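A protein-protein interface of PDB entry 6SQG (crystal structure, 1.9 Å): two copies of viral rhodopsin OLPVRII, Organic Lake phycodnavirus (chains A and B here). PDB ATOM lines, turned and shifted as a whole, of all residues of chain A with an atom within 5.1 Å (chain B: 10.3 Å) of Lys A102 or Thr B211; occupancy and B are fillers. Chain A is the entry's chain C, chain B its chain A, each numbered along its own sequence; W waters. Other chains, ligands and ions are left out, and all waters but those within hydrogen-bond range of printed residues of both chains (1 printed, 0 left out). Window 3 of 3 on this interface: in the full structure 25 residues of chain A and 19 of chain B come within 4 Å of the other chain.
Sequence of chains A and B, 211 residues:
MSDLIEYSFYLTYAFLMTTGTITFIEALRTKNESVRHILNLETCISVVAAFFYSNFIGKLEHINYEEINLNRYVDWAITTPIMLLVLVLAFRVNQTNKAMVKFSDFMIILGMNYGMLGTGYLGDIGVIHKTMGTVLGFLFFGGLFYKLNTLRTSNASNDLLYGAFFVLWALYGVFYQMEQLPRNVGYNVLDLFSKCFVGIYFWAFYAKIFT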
ATOM      1  N   ARG A  92       9.558  -0.007  26.929  1.00  0.00           N
ATOM      2  CA  ARG A  92       8.453  -0.032  27.864  1.00  0.00           C
ATOM      3  C   ARG A  92       8.483  -1.282  28.731  1.00  0.00           C
ATOM      4  O   ARG A  92       8.172  -1.225  29.928  1.00  0.00           O
ATOM      5  CB  ARG A  92       7.138   0.047  27.105  1.00  0.00           C
ATOM      6  CG  ARG A  92       6.017   0.641  27.921  1.00  0.00           C
ATOM      7  CD  ARG A  92       6.289   2.111  28.191  1.00  0.00           C
ATOM      8  NE  ARG A  92       5.547   2.560  29.356  1.00  0.00           N
ATOM      9  CZ  ARG A  92       4.418   3.250  29.302  1.00  0.00           C
ATOM     10  NH1 ARG A  92       3.903   3.597  28.129  1.00  0.00           N
ATOM     11  NH2 ARG A  92       3.810   3.605  30.426  1.00  0.00           N
ATOM     12  N   MET A 100       3.745  -1.498  25.969  1.00  0.00           N
ATOM     13  CA  MET A 100       2.753  -0.492  25.599  1.00  0.00           C
ATOM     14  C   MET A 100       3.453   0.766  25.114  1.00  0.00           C
ATOM     15  O   MET A 100       4.592   1.039  25.492  1.00  0.00           O
ATOM     16  CB  MET A 100       1.892  -0.103  26.799  1.00  0.00           C
ATOM     17  CG  MET A 100       1.469  -1.247  27.701  1.00  0.00           C
ATOM     18  SD  MET A 100       0.537  -0.630  29.118  1.00  0.00           S
ATOM     19  CE  MET A 100      -1.037  -0.290  28.324  1.00  0.00           C
ATOM     20  N   VAL A 101       2.754   1.547  24.305  1.00  0.00           N
ATOM     21  CA  VAL A 101       3.219   2.875  23.934  1.00  0.00           C
ATOM     22  C   VAL A 101       1.980   3.715  23.651  1.00  0.00           C
ATOM     23  O   VAL A 101       0.929   3.175  23.304  1.00  0.00           O
ATOM     24  CB  VAL A 101       4.145   2.812  22.689  1.00  0.00           C
ATOM     25  CG1 VAL A 101       3.367   2.342  21.467  1.00  0.00           C
ATOM     26  CG2 VAL A 101       4.798   4.159  22.418  1.00  0.00           C
ATOM     27  N   LYS A 102       2.083   5.027  23.812  1.00  0.00           N
ATOM     28  CA  LYS A 102       1.005   5.908  23.395  1.00  0.00           C
ATOM     29  C   LYS A 102       0.946   5.921  21.877  1.00  0.00           C
ATOM     30  O   LYS A 102       1.968   6.106  21.224  1.00  0.00           O
ATOM     31  CB  LYS A 102       1.223   7.327  23.915  1.00  0.00           C
ATOM     32  CG  LYS A 102       0.991   7.501  25.409  1.00  0.00           C
ATOM     33  CD  LYS A 102       0.957   8.979  25.797  1.00  0.00           C
ATOM     34  N   PHE A 103      -0.245   5.721  21.316  1.00  0.00           N
ATOM     35  CA  PHE A 103      -0.418   5.737  19.871  1.00  0.00           C
ATOM     36  C   PHE A 103       0.034   7.055  19.238  1.00  0.00           C
ATOM     37  O   PHE A 103       0.645   7.056  18.168  1.00  0.00           O
ATOM     38  CB  PHE A 103      -1.874   5.445  19.466  1.00  0.00           C
ATOM     39  CG  PHE A 103      -2.049   5.280  17.978  1.00  0.00           C
ATOM     40  CD1 PHE A 103      -1.430   4.231  17.312  1.00  0.00           C
ATOM     41  CD2 PHE A 103      -2.783   6.190  17.240  1.00  0.00           C
ATOM     42  CE1 PHE A 103      -1.563   4.083  15.939  1.00  0.00           C
ATOM     43  CE2 PHE A 103      -2.916   6.048  15.869  1.00  0.00           C
ATOM     44  CZ  PHE A 103      -2.309   4.993  15.216  1.00  0.00           C
ATOM     45  N   SER A 104      -0.273   8.170  19.896  1.00  0.00           N
ATOM     46  CA  SER A 104       0.111   9.485  19.391  1.00  0.00           C
ATOM     47  C   SER A 104       1.627   9.600  19.301  1.00  0.00           C
ATOM     48  O   SER A 104       2.144  10.190  18.358  1.00  0.00           O
ATOM     49  CB  SER A 104      -0.438  10.603  20.291  1.00  0.00           C
ATOM     50  OG  SER A 104      -0.024  10.418  21.640  1.00  0.00           O
ATOM     51  N   ASP A 105       2.333   9.067  20.296  1.00  0.00           N
ATOM     52  CA  ASP A 105       3.799   9.037  20.266  1.00  0.00           C
ATOM     53  C   ASP A 105       4.300   8.197  19.096  1.00  0.00           C
ATOM     54  O   ASP A 105       5.214   8.590  18.392  1.00  0.00           O
ATOM     55  CB  ASP A 105       4.356   8.460  21.557  1.00  0.00           C
ATOM     56  CG  ASP A 105       4.365   9.459  22.693  1.00  0.00           C
ATOM     57  OD1 ASP A 105       4.344  10.674  22.415  1.00  0.00           O
ATOM     58  OD2 ASP A 105       4.410   9.021  23.864  1.00  0.00           O
ATOM     59  N   PHE A 106       3.691   7.035  18.891  1.00  0.00           N
ATOM     60  CA  PHE A 106       4.095   6.163  17.792  1.00  0.00           C
ATOM     61  C   PHE A 106       3.834   6.836  16.448  1.00  0.00           C
ATOM     62  O   PHE A 106       4.638   6.718  15.529  1.00  0.00           O
ATOM     63  CB  PHE A 106       3.367   4.822  17.877  1.00  0.00           C
ATOM     64  CG  PHE A 106       3.815   3.822  16.845  1.00  0.00           C
ATOM     65  CD1 PHE A 106       5.153   3.491  16.715  1.00  0.00           C
ATOM     66  CD2 PHE A 106       2.894   3.199  16.027  1.00  0.00           C
ATOM     67  CE1 PHE A 106       5.564   2.571  15.767  1.00  0.00           C
ATOM     68  CE2 PHE A 106       3.299   2.274  15.073  1.00  0.00           C
ATOM     69  CZ  PHE A 106       4.636   1.962  14.946  1.00  0.00           C
ATOM     70  N   TYR B 201      -4.843  -3.379  13.765  1.00  0.00           N
ATOM     71  CA  TYR B 201      -5.606  -2.734  14.825  1.00  0.00           C
ATOM     72  C   TYR B 201      -6.234  -3.744  15.778  1.00  0.00           C
ATOM     73  O   TYR B 201      -6.127  -3.602  16.999  1.00  0.00           O
ATOM     74  CB  TYR B 201      -6.693  -1.808  14.264  1.00  0.00           C
ATOM     75  CG  TYR B 201      -7.666  -1.341  15.331  1.00  0.00           C
ATOM     76  CD1 TYR B 201      -7.333  -0.316  16.201  1.00  0.00           C
ATOM     77  CD2 TYR B 201      -8.897  -1.957  15.494  1.00  0.00           C
ATOM     78  CE1 TYR B 201      -8.204   0.095  17.196  1.00  0.00           C
ATOM     79  CE2 TYR B 201      -9.776  -1.551  16.476  1.00  0.00           C
ATOM     80  CZ  TYR B 201      -9.432  -0.524  17.324  1.00  0.00           C
ATOM     81  OH  TYR B 201     -10.322  -0.117  18.303  1.00  0.00           O
ATOM     82  N   ALA B 204      -3.474  -5.208  17.857  1.00  0.00           N
ATOM     83  CA  ALA B 204      -2.912  -4.238  18.800  1.00  0.00           C
ATOM     84  C   ALA B 204      -3.923  -3.909  19.897  1.00  0.00           C
ATOM     85  O   ALA B 204      -3.561  -3.710  21.056  1.00  0.00           O
ATOM     86  CB  ALA B 204      -2.501  -2.973  18.069  1.00  0.00           C
ATOM     87  N   PHE B 205      -5.197  -3.866  19.525  1.00  0.00           N
ATOM     88  CA  PHE B 205      -6.246  -3.527  20.462  1.00  0.00           C
ATOM     89  C   PHE B 205      -6.408  -4.614  21.511  1.00  0.00           C
ATOM     90  O   PHE B 205      -6.433  -4.336  22.708  1.00  0.00           O
ATOM     91  CB  PHE B 205      -7.561  -3.321  19.728  1.00  0.00           C
ATOM     92  CG  PHE B 205      -8.688  -2.961  20.629  1.00  0.00           C
ATOM     93  CD1 PHE B 205      -8.757  -1.701  21.194  1.00  0.00           C
ATOM     94  CD2 PHE B 205      -9.678  -3.880  20.921  1.00  0.00           C
ATOM     95  CE1 PHE B 205      -9.801  -1.360  22.038  1.00  0.00           C
ATOM     96  CE2 PHE B 205     -10.720  -3.547  21.761  1.00  0.00           C
ATOM     97  CZ  PHE B 205     -10.782  -2.284  22.320  1.00  0.00           C
ATOM     98  N   ALA B 207      -4.250  -6.975  22.194  1.00  0.00           N
ATOM     99  CA  ALA B 207      -2.969  -7.159  22.874  1.00  0.00           C
ATOM    100  C   ALA B 207      -2.651  -6.022  23.858  1.00  0.00           C
ATOM    101  O   ALA B 207      -1.699  -6.127  24.627  1.00  0.00           O
ATOM    102  CB  ALA B 207      -1.848  -7.287  21.855  1.00  0.00           C
ATOM    103  N   LYS B 208      -3.445  -4.953  23.821  1.00  0.00           N
ATOM    104  CA  LYS B 208      -3.278  -3.780  24.698  1.00  0.00           C
ATOM    105  C   LYS B 208      -1.920  -3.112  24.493  1.00  0.00           C
ATOM    106  O   LYS B 208      -1.252  -2.716  25.444  1.00  0.00           O
ATOM    107  CB  LYS B 208      -3.493  -4.155  26.163  1.00  0.00           C
ATOM    108  CG  LYS B 208      -4.925  -4.566  26.468  1.00  0.00           C
ATOM    109  CD  LYS B 208      -5.069  -5.100  27.886  1.00  0.00           C
ATOM    110  N   ILE B 209      -1.548  -2.977  23.225  1.00  0.00           N
ATOM    111  CA  ILE B 209      -0.255  -2.450  22.812  1.00  0.00           C
ATOM    112  C   ILE B 209      -0.233  -0.926  22.942  1.00  0.00           C
ATOM    113  O   ILE B 209       0.811  -0.332  23.221  1.00  0.00           O
ATOM    114  CB  ILE B 209       0.020  -2.871  21.343  1.00  0.00           C
ATOM    115  CG1 ILE B 209       0.289  -4.376  21.273  1.00  0.00           C
ATOM    116  CG2 ILE B 209       1.186  -2.113  20.735  1.00  0.00           C
ATOM    117  CD1 ILE B 209       1.431  -4.832  22.155  1.00  0.00           C
ATOM    118  N   PHE B 210      -1.387  -0.299  22.747  1.00  0.00           N
ATOM    119  CA  PHE B 210      -1.462   1.157  22.755  1.00  0.00           C
ATOM    120  C   PHE B 210      -2.248   1.676  23.946  1.00  0.00           C
ATOM    121  O   PHE B 210      -3.245   1.087  24.337  1.00  0.00           O
ATOM    122  CB  PHE B 210      -2.082   1.669  21.457  1.00  0.00           C
ATOM    123  CG  PHE B 210      -1.249   1.383  20.246  1.00  0.00           C
ATOM    124  CD1 PHE B 210       0.041   1.880  20.151  1.00  0.00           C
ATOM    125  CD2 PHE B 210      -1.740   0.604  19.214  1.00  0.00           C
ATOM    126  CE1 PHE B 210       0.823   1.614  19.043  1.00  0.00           C
ATOM    127  CE2 PHE B 210      -0.965   0.339  18.100  1.00  0.00           C
ATOM    128  CZ  PHE B 210       0.322   0.838  18.020  1.00  0.00           C
ATOM    129  N   THR B 211      -1.763   2.766  24.535  1.00  0.00           N
ATOM    130  CA  THR B 211      -2.536   3.530  25.511  1.00  0.00           C
ATOM    131  C   THR B 211      -3.198   4.716  24.803  1.00  0.00           C
ATOM    132  O   THR B 211      -2.720   5.176  23.751  1.00  0.00           O
ATOM    133  CB  THR B 211      -1.650   4.052  26.661  1.00  0.00           C
ATOM    134  OG1 THR B 211      -0.589   4.850  26.127  1.00  0.00           O
ATOM    135  CG2 THR B 211      -1.056   2.903  27.451  1.00  0.00           C
HETATM  136  O   HOH W   1      -2.292   8.254  22.250  1.00  0.00           O
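O of Ala B204 lies within hydrogen-bond range of N of Ile B209 (3.0 Å).
Among the printed residues, merely in contact across the chains: Met A100 with Lys B208 (3.8 Å), Met A100 with Ile B209 (3.1 Å), Met A100 with Thr B211 (3.3 Å), Val A101 with Phe B210 (3.2 Å), Lys A102 with Thr B211 (3.2 Å), Phe A103 with Phe B210 (3.9 Å), Phe A103 with Thr B211 (3.5 Å) and Phe A106 with Phe B210 (3.99 Å).
The backbone NH of Val A101 sits at hydrogen-bond distance from the backbone carbonyl oxygen of Ile B209 (2.9 Å).
The backbone NH of Thr B211 is in hydrogen-bond range of the backbone carbonyl oxygen of Val A101 (3.0 Å).
Water W1 lies within hydrogen-bond range of N of Ser A104 (3.1 Å), N of Phe A103 (3.4 Å) and O of Thr B211 (3.5 Å).
Of the 8 printed residues of chain B, 4 touch a printed residue of chain A.
Hydrophobic or aromatic side chains of chain B within 4 Å of the printed part of chain A: Phe B210.
Hydrophobic or aromatic side chains of chain A that line the printed part of chain B: Met A100, Val A101, Phe A103 and Phe A106.
Among the printed residues, no Asp or Glu carboxylate lies within 4 Å of a Lys or Arg side-chain nitrogen of the other chain.
No position is printed for both chains.
Of the 10 pairs that touch across the chains among the printed residues, none has its exchanged pair printed and touching as well.
Lys A102 touches one residue of chain B.
Thr B211 touches just these residues of chain A: Met A100, Val A101, Lys A102 and Phe A103.
Of the printed residues of chain B, Val A101 touches Ile B209, Phe B210 and Thr B211.
No residue of chain B comes within 4 Å of Ser A104.
Printed residues of chain B within 4 Å of Met A100: Lys B208 (3.8 Å), Ile B209 (3.1 Å) and Thr B211 (3.3 Å).
Of the printed residues of chain A, Ile B209 touches Met A100 (3.1 Å) and Val A101 (2.9 Å).
Of the printed residues of chain B, Phe A103 touches Phe B210 and Thr B211.
Of the printed residues of chain B, Phe A106 touches Phe B210 (3.99 Å).
Ala B207 touches none of the printed residues of chain A.
The nearest residue of chain B that does not touch Lys A102 is Phe B210 (4.5 Å).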
